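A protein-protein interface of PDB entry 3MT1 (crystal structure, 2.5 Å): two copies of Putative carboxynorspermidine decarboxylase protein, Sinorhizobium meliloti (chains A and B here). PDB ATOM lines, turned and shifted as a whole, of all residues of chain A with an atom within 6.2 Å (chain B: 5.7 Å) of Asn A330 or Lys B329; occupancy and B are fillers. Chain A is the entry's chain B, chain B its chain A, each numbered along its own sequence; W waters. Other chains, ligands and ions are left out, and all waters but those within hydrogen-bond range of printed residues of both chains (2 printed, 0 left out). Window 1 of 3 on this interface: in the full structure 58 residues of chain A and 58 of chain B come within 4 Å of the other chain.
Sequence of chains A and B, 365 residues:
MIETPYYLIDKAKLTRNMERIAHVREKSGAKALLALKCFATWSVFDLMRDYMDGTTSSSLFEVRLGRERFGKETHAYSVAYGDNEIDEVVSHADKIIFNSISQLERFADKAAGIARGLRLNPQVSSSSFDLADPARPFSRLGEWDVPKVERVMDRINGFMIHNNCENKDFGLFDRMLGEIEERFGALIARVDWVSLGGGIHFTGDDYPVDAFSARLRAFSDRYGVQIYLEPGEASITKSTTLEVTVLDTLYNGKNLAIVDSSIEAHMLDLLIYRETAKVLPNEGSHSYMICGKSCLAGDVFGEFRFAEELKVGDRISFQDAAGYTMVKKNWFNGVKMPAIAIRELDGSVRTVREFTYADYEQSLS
The backbone carbonyl oxygen (O) of Val B327 lies within hydrogen-bond range of the backbone NH (N) of Phe A332, at 3.5 Å.
NZ of Lys B328 is in salt-bridge range of OE2 of Glu A264.
The backbone carbonyl oxygen of Ser A363 is in hydrogen-bond range of the side-chain amino group of Lys B329 (2.7 Å).
The backbone carbonyl oxygen of Ala B265 is in hydrogen-bond range of the backbone NH of Asn B330, at 3.0 Å.
The backbone carbonyl oxygen (O) of Lys B328 lies within hydrogen-bond range of the side-chain amide nitrogen (ND2) of Asn B330 (3.4 Å).
The backbone carbonyl oxygen (O) of Glu A264 lies within hydrogen-bond range of the side-chain amide nitrogen (ND2) of Asn A330, 3.0 Å away.
The backbone carbonyl oxygen of Lys A328 lies within hydrogen-bond range of the side-chain amide nitrogen of Asn A330, at 3.4 Å.
The side-chain sulfur of Met A337 sits at hydrogen-bond distance from the side-chain amino group of Lys A329.
OD1 of Asn A330 lies close to N of Phe A332, at 3.1 Å.
Among the printed residues, merely in contact across the chains: Leu A268 with Leu B268 (3.8 Å), Lys A328 with Asn B330 (3.7 Å), Lys A329 with Asn B330 (3.7 Å), Asn A330 with Lys B328 (3.7 Å), Asn A330 with Lys B329 (3.7 Å), Trp A331 with Val B327 (3.6 Å), Phe A332 with Lys B328 (3.5 Å), Ser A363 with Phe B355 (3.5 Å) and Leu A364 with Ile B340 (3.5 Å).
Asn A330 touches just these residues of chain B: Lys B328 and Lys B329.
Of the printed residues of chain B, Trp A331 touches Val B327 (3.6 Å).
Printed residues of chain A within 4 Å of Asn B330: Lys A328 (3.7 Å) and Lys A329 (3.7 Å).
His A266 touches none of the printed residues of chain B.
Gln A362 touches none of the printed residues of chain B.
The nearest residue of chain A that does not touch Lys B329 is Lys A329 (4.8 Å).
Of the 15 printed residues of chain A, 9 touch a printed residue of chain B.
Hydrophobic or aromatic side chains of chain A that line the printed part of chain B: Leu A268 and Phe A332.
Hydrophobic or aromatic side chains of chain B that line the printed part of chain A: Leu B268, Ile B340 and Phe B355.
Among the printed residues, Asp or Glu carboxylates within 4 Å of a Lys or Arg side-chain nitrogen of the other chain: Glu A264 with Lys B328 (2.7 Å).
Leu A268 touches its own counterpart, Leu B268.
Lys A328 touches Asn B330, and with the chains exchanged Asn A330 touches Lys B328.
Lys A329 touches Asn B330, and with the chains exchanged Asn A330 touches Lys B329.
Positions printed for both chains: 265, 266, 268, 328, 329, 330, 331 and 337.
Of the 12 pairs that touch across the chains among the printed residues, 5 have their exchanged pair printed and touching as well.
Water W2 bridges the backbone carbonyl oxygen of Lys A329 (2.6 Å) and the backbone NH of Trp B331 (3.0 Å).
Water W1 lies within hydrogen-bond range of the backbone NH of Trp A331 (2.8 Å) and the backbone carbonyl oxygen of Lys B329 (2.8 Å).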
ATOM      1  N   GLU A 264     -33.909   8.152 -18.760  1.00  0.00           N
ATOM      2  CA  GLU A 264     -32.868   8.309 -17.767  1.00  0.00           C
ATOM      3  C   GLU A 264     -32.471   6.966 -17.166  1.00  0.00           C
ATOM      4  O   GLU A 264     -31.285   6.704 -16.916  1.00  0.00           O
ATOM      5  CB  GLU A 264     -33.223   9.325 -16.656  1.00  0.00           C
ATOM      6  CG  GLU A 264     -32.023   9.535 -15.736  1.00  0.00           C
ATOM      7  CD  GLU A 264     -32.141  10.727 -14.819  1.00  0.00           C
ATOM      8  OE1 GLU A 264     -32.965  11.607 -15.098  1.00  0.00           O
ATOM      9  OE2 GLU A 264     -31.432  10.775 -13.798  1.00  0.00           O
ATOM     10  N   ALA A 265     -33.463   6.108 -16.967  1.00  0.00           N
ATOM     11  CA  ALA A 265     -33.231   4.863 -16.259  1.00  0.00           C
ATOM     12  C   ALA A 265     -32.825   3.750 -17.199  1.00  0.00           C
ATOM     13  O   ALA A 265     -32.186   2.794 -16.771  1.00  0.00           O
ATOM     14  CB  ALA A 265     -34.468   4.460 -15.490  1.00  0.00           C
ATOM     15  N   HIS A 266     -33.214   3.858 -18.461  1.00  0.00           N
ATOM     16  CA  HIS A 266     -33.218   2.680 -19.363  1.00  0.00           C
ATOM     17  C   HIS A 266     -32.428   2.811 -20.649  1.00  0.00           C
ATOM     18  O   HIS A 266     -32.085   1.804 -21.241  1.00  0.00           O
ATOM     19  CB  HIS A 266     -34.649   2.231 -19.674  1.00  0.00           C
ATOM     20  CG  HIS A 266     -35.463   2.002 -18.443  1.00  0.00           C
ATOM     21  ND1 HIS A 266     -36.823   2.219 -18.389  1.00  0.00           N
ATOM     22  CD2 HIS A 266     -35.094   1.599 -17.198  1.00  0.00           C
ATOM     23  CE1 HIS A 266     -37.259   1.941 -17.171  1.00  0.00           C
ATOM     24  NE2 HIS A 266     -36.229   1.572 -16.427  1.00  0.00           N
ATOM     25  N   LEU A 268     -29.814   5.631 -21.198  1.00  0.00           N
ATOM     26  CA  LEU A 268     -29.303   6.827 -20.604  1.00  0.00           C
ATOM     27  C   LEU A 268     -28.444   7.619 -21.576  1.00  0.00           C
ATOM     28  O   LEU A 268     -28.353   8.836 -21.472  1.00  0.00           O
ATOM     29  CB  LEU A 268     -28.553   6.462 -19.321  1.00  0.00           C
ATOM     30  CG  LEU A 268     -27.663   7.483 -18.582  1.00  0.00           C
ATOM     31  CD1 LEU A 268     -28.464   8.694 -18.050  1.00  0.00           C
ATOM     32  CD2 LEU A 268     -26.821   6.838 -17.448  1.00  0.00           C
ATOM     33  N   LYS A 328     -25.888   0.412 -18.081  1.00  0.00           N
ATOM     34  CA  LYS A 328     -25.931   1.651 -17.339  1.00  0.00           C
ATOM     35  C   LYS A 328     -27.340   1.974 -16.873  1.00  0.00           C
ATOM     36  O   LYS A 328     -27.634   3.091 -16.504  1.00  0.00           O
ATOM     37  CB  LYS A 328     -25.255   2.806 -18.100  1.00  0.00           C
ATOM     38  CG  LYS A 328     -25.738   3.032 -19.535  1.00  0.00           C
ATOM     39  CD  LYS A 328     -25.119   4.325 -20.107  1.00  0.00           C
ATOM     40  CE  LYS A 328     -23.976   4.017 -21.040  1.00  0.00           C
ATOM     41  NZ  LYS A 328     -23.026   5.122 -21.155  1.00  0.00           N
ATOM     42  N   LYS A 329     -28.196   0.967 -16.853  1.00  0.00           N
ATOM     43  CA  LYS A 329     -29.531   1.148 -16.342  1.00  0.00           C
ATOM     44  C   LYS A 329     -29.537   1.379 -14.843  1.00  0.00           C
ATOM     45  O   LYS A 329     -28.681   0.876 -14.110  1.00  0.00           O
ATOM     46  CB  LYS A 329     -30.385  -0.052 -16.706  1.00  0.00           C
ATOM     47  CG  LYS A 329     -29.927  -1.392 -16.131  1.00  0.00           C
ATOM     48  CD  LYS A 329     -30.853  -2.523 -16.643  1.00  0.00           C
ATOM     49  CE  LYS A 329     -30.133  -3.890 -16.597  1.00  0.00           C
ATOM     50  NZ  LYS A 329     -29.590  -4.084 -15.218  1.00  0.00           N
ATOM     51  N   ASN A 330     -30.514   2.133 -14.376  1.00  0.00           N
ATOM     52  CA  ASN A 330     -30.576   2.481 -12.959  1.00  0.00           C
ATOM     53  C   ASN A 330     -32.039   2.571 -12.426  1.00  0.00           C
ATOM     54  O   ASN A 330     -33.019   2.446 -13.193  1.00  0.00           O
ATOM     55  CB  ASN A 330     -29.842   3.801 -12.766  1.00  0.00           C
ATOM     56  CG  ASN A 330     -30.418   4.883 -13.630  1.00  0.00           C
ATOM     57  OD1 ASN A 330     -31.422   5.499 -13.265  1.00  0.00           O
ATOM     58  ND2 ASN A 330     -29.828   5.094 -14.817  1.00  0.00           N
ATOM     59  N   TRP A 331     -32.165   2.852 -11.129  1.00  0.00           N
ATOM     60  CA  TRP A 331     -33.439   2.843 -10.426  1.00  0.00           C
ATOM     61  C   TRP A 331     -34.021   4.244 -10.226  1.00  0.00           C
ATOM     62  O   TRP A 331     -34.791   4.495  -9.303  1.00  0.00           O
ATOM     63  CB  TRP A 331     -33.200   2.227  -9.072  1.00  0.00           C
ATOM     64  CG  TRP A 331     -33.113   0.780  -9.113  1.00  0.00           C
ATOM     65  CD1 TRP A 331     -32.028   0.023  -8.809  1.00  0.00           C
ATOM     66  CD2 TRP A 331     -34.162  -0.128  -9.486  1.00  0.00           C
ATOM     67  NE1 TRP A 331     -32.336  -1.307  -8.959  1.00  0.00           N
ATOM     68  CE2 TRP A 331     -33.638  -1.432  -9.364  1.00  0.00           C
ATOM     69  CE3 TRP A 331     -35.495   0.036  -9.896  1.00  0.00           C
ATOM     70  CZ2 TRP A 331     -34.402  -2.578  -9.646  1.00  0.00           C
ATOM     71  CZ3 TRP A 331     -36.260  -1.096 -10.170  1.00  0.00           C
ATOM     72  CH2 TRP A 331     -35.720  -2.386 -10.038  1.00  0.00           C
ATOM     73  N   PHE A 332     -33.629   5.176 -11.094  1.00  0.00           N
ATOM     74  CA  PHE A 332     -34.152   6.516 -11.042  1.00  0.00           C
ATOM     75  C   PHE A 332     -35.678   6.524 -10.931  1.00  0.00           C
ATOM     76  O   PHE A 332     -36.380   5.834 -11.709  1.00  0.00           O
ATOM     77  CB  PHE A 332     -33.749   7.191 -12.312  1.00  0.00           C
ATOM     78  CG  PHE A 332     -34.264   8.578 -12.444  1.00  0.00           C
ATOM     79  CD1 PHE A 332     -33.845   9.580 -11.563  1.00  0.00           C
ATOM     80  CD2 PHE A 332     -35.166   8.890 -13.454  1.00  0.00           C
ATOM     81  CE1 PHE A 332     -34.321  10.883 -11.693  1.00  0.00           C
ATOM     82  CE2 PHE A 332     -35.642  10.207 -13.600  1.00  0.00           C
ATOM     83  CZ  PHE A 332     -35.210  11.196 -12.729  1.00  0.00           C
ATOM     84  N   ASN A 333     -36.173   7.292  -9.958  1.00  0.00           N
ATOM     85  CA  ASN A 333     -37.597   7.421  -9.646  1.00  0.00           C
ATOM     86  C   ASN A 333     -38.224   6.144  -9.066  1.00  0.00           C
ATOM     87  O   ASN A 333     -39.410   6.113  -8.775  1.00  0.00           O
ATOM     88  CB  ASN A 333     -38.398   7.920 -10.881  1.00  0.00           C
ATOM     89  CG  ASN A 333     -38.520   9.471 -10.947  1.00  0.00           C
ATOM     90  OD1 ASN A 333     -37.615  10.204 -10.533  1.00  0.00           O
ATOM     91  ND2 ASN A 333     -39.653   9.958 -11.473  1.00  0.00           N
ATOM     92  N   VAL A 335     -38.719   3.749 -10.929  1.00  0.00           N
ATOM     93  CA  VAL A 335     -39.432   3.083 -12.023  1.00  0.00           C
ATOM     94  C   VAL A 335     -38.948   1.652 -12.254  1.00  0.00           C
ATOM     95  O   VAL A 335     -37.784   1.316 -12.024  1.00  0.00           O
ATOM     96  CB  VAL A 335     -39.540   3.873 -13.378  1.00  0.00           C
ATOM     97  CG1 VAL A 335     -40.037   5.288 -13.151  1.00  0.00           C
ATOM     98  CG2 VAL A 335     -38.242   3.848 -14.133  1.00  0.00           C
ATOM     99  N   MET A 337     -37.548  -1.610 -13.586  1.00  0.00           N
ATOM    100  CA  MET A 337     -36.433  -1.839 -14.441  1.00  0.00           C
ATOM    101  C   MET A 337     -36.784  -2.882 -15.525  1.00  0.00           C
ATOM    102  O   MET A 337     -37.476  -3.847 -15.252  1.00  0.00           O
ATOM    103  CB  MET A 337     -35.237  -2.277 -13.601  1.00  0.00           C
ATOM    104  CG  MET A 337     -33.915  -2.313 -14.373  1.00  0.00           C
ATOM    105  SD  MET A 337     -32.497  -2.785 -13.153  1.00  0.00           S
ATOM    106  CE  MET A 337     -32.046  -0.986 -12.518  1.00  0.00           C
ATOM    107  N   GLN A 362     -32.674  -3.357  -2.169  1.00  0.00           N
ATOM    108  CA  GLN A 362     -31.294  -3.759  -1.914  1.00  0.00           C
ATOM    109  C   GLN A 362     -30.231  -2.868  -2.597  1.00  0.00           C
ATOM    110  O   GLN A 362     -29.055  -2.890  -2.222  1.00  0.00           O
ATOM    111  CB  GLN A 362     -31.104  -5.245  -2.281  1.00  0.00           C
ATOM    112  CG  GLN A 362     -31.723  -6.161  -1.232  1.00  0.00           C
ATOM    113  CD  GLN A 362     -32.054  -7.546  -1.758  1.00  0.00           C
ATOM    114  OE1 GLN A 362     -31.682  -7.920  -2.870  1.00  0.00           O
ATOM    115  NE2 GLN A 362     -32.786  -8.311  -0.964  1.00  0.00           N
ATOM    116  N   SER A 363     -30.628  -2.068  -3.567  1.00  0.00           N
ATOM    117  CA  SER A 363     -29.680  -1.130  -4.116  1.00  0.00           C
ATOM    118  C   SER A 363     -29.545   0.151  -3.272  1.00  0.00           C
ATOM    119  O   SER A 363     -28.639   0.932  -3.509  1.00  0.00           O
ATOM    120  CB  SER A 363     -30.041  -0.781  -5.556  1.00  0.00           C
ATOM    121  OG  SER A 363     -31.184   0.040  -5.556  1.00  0.00           O
ATOM    122  N   LEU A 364     -30.399   0.346  -2.265  1.00  0.00           N
ATOM    123  CA  LEU A 364     -30.458   1.632  -1.520  1.00  0.00           C
ATOM    124  C   LEU A 364     -29.921   1.564  -0.108  1.00  0.00           C
ATOM    125  O   LEU A 364     -29.690   2.569   0.533  1.00  0.00           O
ATOM    126  CB  LEU A 364     -31.899   2.157  -1.444  1.00  0.00           C
ATOM    127  CG  LEU A 364     -32.299   2.785  -2.769  1.00  0.00           C
ATOM    128  CD1 LEU A 364     -33.805   2.948  -2.884  1.00  0.00           C
ATOM    129  CD2 LEU A 364     -31.496   4.104  -3.039  1.00  0.00           C
ATOM    130  N   TYR B   7     -20.339   6.472  -0.284  1.00  0.00           N
ATOM    131  CA  TYR B   7     -21.095   7.623   0.220  1.00  0.00           C
ATOM    132  C   TYR B   7     -21.101   7.560   1.735  1.00  0.00           C
ATOM    133  O   TYR B   7     -21.292   6.477   2.320  1.00  0.00           O
ATOM    134  CB  TYR B   7     -22.518   7.616  -0.272  1.00  0.00           C
ATOM    135  CG  TYR B   7     -22.642   7.576  -1.759  1.00  0.00           C
ATOM    136  CD1 TYR B   7     -22.816   6.370  -2.424  1.00  0.00           C
ATOM    137  CD2 TYR B   7     -22.588   8.750  -2.522  1.00  0.00           C
ATOM    138  CE1 TYR B   7     -22.961   6.318  -3.801  1.00  0.00           C
ATOM    139  CE2 TYR B   7     -22.736   8.706  -3.926  1.00  0.00           C
ATOM    140  CZ  TYR B   7     -22.912   7.471  -4.544  1.00  0.00           C
ATOM    141  OH  TYR B   7     -23.049   7.398  -5.909  1.00  0.00           O
ATOM    142  N   ALA B 265     -21.360   7.103 -13.327  1.00  0.00           N
ATOM    143  CA  ALA B 265     -21.831   6.030 -12.502  1.00  0.00           C
ATOM    144  C   ALA B 265     -22.339   6.515 -11.165  1.00  0.00           C
ATOM    145  O   ALA B 265     -23.203   5.906 -10.588  1.00  0.00           O
ATOM    146  CB  ALA B 265     -20.711   5.026 -12.296  1.00  0.00           C
ATOM    147  N   HIS B 266     -21.801   7.612 -10.662  1.00  0.00           N
ATOM    148  CA  HIS B 266     -21.956   7.894  -9.251  1.00  0.00           C
ATOM    149  C   HIS B 266     -22.440   9.272  -8.957  1.00  0.00           C
ATOM    150  O   HIS B 266     -22.775   9.551  -7.808  1.00  0.00           O
ATOM    151  CB  HIS B 266     -20.635   7.702  -8.485  1.00  0.00           C
ATOM    152  CG  HIS B 266     -19.991   6.381  -8.728  1.00  0.00           C
ATOM    153  ND1 HIS B 266     -18.618   6.221  -8.773  1.00  0.00           N
ATOM    154  CD2 HIS B 266     -20.529   5.157  -8.961  1.00  0.00           C
ATOM    155  CE1 HIS B 266     -18.340   4.955  -9.019  1.00  0.00           C
ATOM    156  NE2 HIS B 266     -19.480   4.285  -9.139  1.00  0.00           N
ATOM    157  N   LEU B 268     -24.389  11.203 -11.541  1.00  0.00           N
ATOM    158  CA  LEU B 268     -24.885  11.371 -12.868  1.00  0.00           C
ATOM    159  C   LEU B 268     -25.452  12.771 -13.176  1.00  0.00           C
ATOM    160  O   LEU B 268     -25.348  13.248 -14.305  1.00  0.00           O
ATOM    161  CB  LEU B 268     -25.897  10.250 -13.104  1.00  0.00           C
ATOM    162  CG  LEU B 268     -26.672  10.048 -14.388  1.00  0.00           C
ATOM    163  CD1 LEU B 268     -25.715   9.875 -15.525  1.00  0.00           C
ATOM    164  CD2 LEU B 268     -27.639   8.859 -14.263  1.00  0.00           C
ATOM    165  N   THR B 325     -28.246  11.117  -6.170  1.00  0.00           N
ATOM    166  CA  THR B 325     -27.029  10.448  -6.585  1.00  0.00           C
ATOM    167  C   THR B 325     -27.117   8.930  -6.377  1.00  0.00           C
ATOM    168  O   THR B 325     -26.998   8.174  -7.344  1.00  0.00           O
ATOM    169  CB  THR B 325     -25.810  10.954  -5.802  1.00  0.00           C
ATOM    170  OG1 THR B 325     -26.057  10.778  -4.399  1.00  0.00           O
ATOM    171  CG2 THR B 325     -25.528  12.425  -6.112  1.00  0.00           C
ATOM    172  N   MET B 326     -27.296   8.492  -5.121  1.00  0.00           N
ATOM    173  CA  MET B 326     -27.397   7.076  -4.806  1.00  0.00           C
ATOM    174  C   MET B 326     -28.611   6.485  -5.479  1.00  0.00           C
ATOM    175  O   MET B 326     -28.688   5.287  -5.716  1.00  0.00           O
ATOM    176  CB  MET B 326     -27.540   6.847  -3.320  1.00  0.00           C
ATOM    177  CG  MET B 326     -26.236   6.708  -2.630  1.00  0.00           C
ATOM    178  SD  MET B 326     -26.364   6.910  -0.671  1.00  0.00           S
ATOM    179  CE  MET B 326     -26.537   8.836  -0.668  1.00  0.00           C
ATOM    180  N   VAL B 327     -29.559   7.338  -5.778  1.00  0.00           N
ATOM    181  CA  VAL B 327     -30.813   6.912  -6.301  1.00  0.00           C
ATOM    182  C   VAL B 327     -30.671   6.622  -7.824  1.00  0.00           C
ATOM    183  O   VAL B 327     -31.597   6.227  -8.499  1.00  0.00           O
ATOM    184  CB  VAL B 327     -31.805   8.051  -5.947  1.00  0.00           C
ATOM    185  CG1 VAL B 327     -32.623   8.453  -7.087  1.00  0.00           C
ATOM    186  CG2 VAL B 327     -32.624   7.672  -4.714  1.00  0.00           C
ATOM    187  N   LYS B 328     -29.499   6.849  -8.375  1.00  0.00           N
ATOM    188  CA  LYS B 328     -29.357   6.687  -9.806  1.00  0.00           C
ATOM    189  C   LYS B 328     -27.943   6.268 -10.202  1.00  0.00           C
ATOM    190  O   LYS B 328     -27.551   6.393 -11.360  1.00  0.00           O
ATOM    191  CB  LYS B 328     -29.798   7.944 -10.550  1.00  0.00           C
ATOM    192  CG  LYS B 328     -28.978   9.178 -10.207  1.00  0.00           C
ATOM    193  CD  LYS B 328     -29.421  10.266 -11.182  1.00  0.00           C
ATOM    194  CE  LYS B 328     -30.421  11.189 -10.541  1.00  0.00           C
ATOM    195  NZ  LYS B 328     -31.044  12.089 -11.526  1.00  0.00           N
ATOM    196  N   LYS B 329     -27.213   5.752  -9.226  1.00  0.00           N
ATOM    197  CA  LYS B 329     -25.922   5.196  -9.467  1.00  0.00           C
ATOM    198  C   LYS B 329     -26.127   3.948 -10.323  1.00  0.00           C
ATOM    199  O   LYS B 329     -27.210   3.265 -10.256  1.00  0.00           O
ATOM    200  CB  LYS B 329     -25.284   4.819  -8.132  1.00  0.00           C
ATOM    201  CG  LYS B 329     -26.186   3.936  -7.292  1.00  0.00           C
ATOM    202  CD  LYS B 329     -25.500   3.444  -5.999  1.00  0.00           C
ATOM    203  CE  LYS B 329     -26.487   2.882  -5.024  1.00  0.00           C
ATOM    204  NZ  LYS B 329     -27.313   1.842  -5.694  1.00  0.00           N
ATOM    205  N   ASN B 330     -25.100   3.652 -11.114  1.00  0.00           N
ATOM    206  CA  ASN B 330     -25.155   2.522 -12.019  1.00  0.00           C
ATOM    207  C   ASN B 330     -23.794   1.819 -12.188  1.00  0.00           C
ATOM    208  O   ASN B 330     -22.816   2.185 -11.543  1.00  0.00           O
ATOM    209  CB  ASN B 330     -25.708   2.997 -13.360  1.00  0.00           C
ATOM    210  CG  ASN B 330     -24.908   4.148 -13.913  1.00  0.00           C
ATOM    211  OD1 ASN B 330     -23.803   3.960 -14.427  1.00  0.00           O
ATOM    212  ND2 ASN B 330     -25.438   5.358 -13.762  1.00  0.00           N
ATOM    213  N   TRP B 331     -23.745   0.817 -13.063  1.00  0.00           N
ATOM    214  CA  TRP B 331     -22.545  -0.002 -13.242  1.00  0.00           C
ATOM    215  C   TRP B 331     -21.783   0.379 -14.503  1.00  0.00           C
ATOM    216  O   TRP B 331     -21.158  -0.461 -15.154  1.00  0.00           O
ATOM    217  CB  TRP B 331     -22.912  -1.489 -13.264  1.00  0.00           C
ATOM    218  CG  TRP B 331     -23.277  -2.051 -11.913  1.00  0.00           C
ATOM    219  CD1 TRP B 331     -24.517  -2.423 -11.495  1.00  0.00           C
ATOM    220  CD2 TRP B 331     -22.394  -2.267 -10.800  1.00  0.00           C
ATOM    221  NE1 TRP B 331     -24.463  -2.866 -10.201  1.00  0.00           N
ATOM    222  CE2 TRP B 331     -23.177  -2.798  -9.750  1.00  0.00           C
ATOM    223  CE3 TRP B 331     -21.013  -2.085 -10.601  1.00  0.00           C
ATOM    224  CZ2 TRP B 331     -22.637  -3.168  -8.509  1.00  0.00           C
ATOM    225  CZ3 TRP B 331     -20.454  -2.452  -9.359  1.00  0.00           C
ATOM    226  CH2 TRP B 331     -21.277  -2.992  -8.321  1.00  0.00           C
ATOM    227  N   MET B 337     -18.892   0.166  -7.373  1.00  0.00           N
ATOM    228  CA  MET B 337     -19.950   1.011  -6.916  1.00  0.00           C
ATOM    229  C   MET B 337     -19.592   1.374  -5.472  1.00  0.00           C
ATOM    230  O   MET B 337     -19.019   0.549  -4.721  1.00  0.00           O
ATOM    231  CB  MET B 337     -21.307   0.287  -7.083  1.00  0.00           C
ATOM    232  CG  MET B 337     -22.594   1.072  -6.697  1.00  0.00           C
ATOM    233  SD  MET B 337     -24.193  -0.026  -7.024  1.00  0.00           S
ATOM    234  CE  MET B 337     -24.477   0.422  -8.921  1.00  0.00           C
ATOM    235  N   PRO B 338     -19.879   2.624  -5.088  1.00  0.00           N
ATOM    236  CA  PRO B 338     -19.454   3.105  -3.779  1.00  0.00           C
ATOM    237  C   PRO B 338     -20.313   2.513  -2.684  1.00  0.00           C
ATOM    238  O   PRO B 338     -21.562   2.416  -2.838  1.00  0.00           O
ATOM    239  CB  PRO B 338     -19.659   4.626  -3.867  1.00  0.00           C
ATOM    240  CG  PRO B 338     -20.141   4.909  -5.259  1.00  0.00           C
ATOM    241  CD  PRO B 338     -20.720   3.609  -5.776  1.00  0.00           C
ATOM    242  N   ILE B 340     -22.381   2.274   0.795  1.00  0.00           N
ATOM    243  CA  ILE B 340     -23.182   3.207   1.558  1.00  0.00           C
ATOM    244  C   ILE B 340     -22.793   3.064   3.014  1.00  0.00           C
ATOM    245  O   ILE B 340     -22.779   1.968   3.545  1.00  0.00           O
ATOM    246  CB  ILE B 340     -24.667   2.912   1.373  1.00  0.00           C
ATOM    247  CG1 ILE B 340     -25.053   3.206  -0.097  1.00  0.00           C
ATOM    248  CG2 ILE B 340     -25.517   3.684   2.400  1.00  0.00           C
ATOM    249  CD1 ILE B 340     -26.411   2.675  -0.537  1.00  0.00           C
ATOM    250  N   PHE B 355     -21.270  -3.174  -2.315  1.00  0.00           N
ATOM    251  CA  PHE B 355     -21.673  -3.759  -3.562  1.00  0.00           C
ATOM    252  C   PHE B 355     -20.514  -4.604  -4.060  1.00  0.00           C
ATOM    253  O   PHE B 355     -19.367  -4.164  -4.030  1.00  0.00           O
ATOM    254  CB  PHE B 355     -22.040  -2.666  -4.549  1.00  0.00           C
ATOM    255  CG  PHE B 355     -23.211  -1.857  -4.125  1.00  0.00           C
ATOM    256  CD1 PHE B 355     -23.047  -0.610  -3.569  1.00  0.00           C
ATOM    257  CD2 PHE B 355     -24.491  -2.357  -4.256  1.00  0.00           C
ATOM    258  CE1 PHE B 355     -24.160   0.148  -3.152  1.00  0.00           C
ATOM    259  CE2 PHE B 355     -25.606  -1.628  -3.850  1.00  0.00           C
ATOM    260  CZ  PHE B 355     -25.445  -0.367  -3.299  1.00  0.00           C
HETATM  261  O   HOH W   1     -29.920   3.174  -9.504  1.00  0.00           O
HETATM  262  O   HOH W   2     -26.303  -0.080 -14.450  1.00  0.00           O
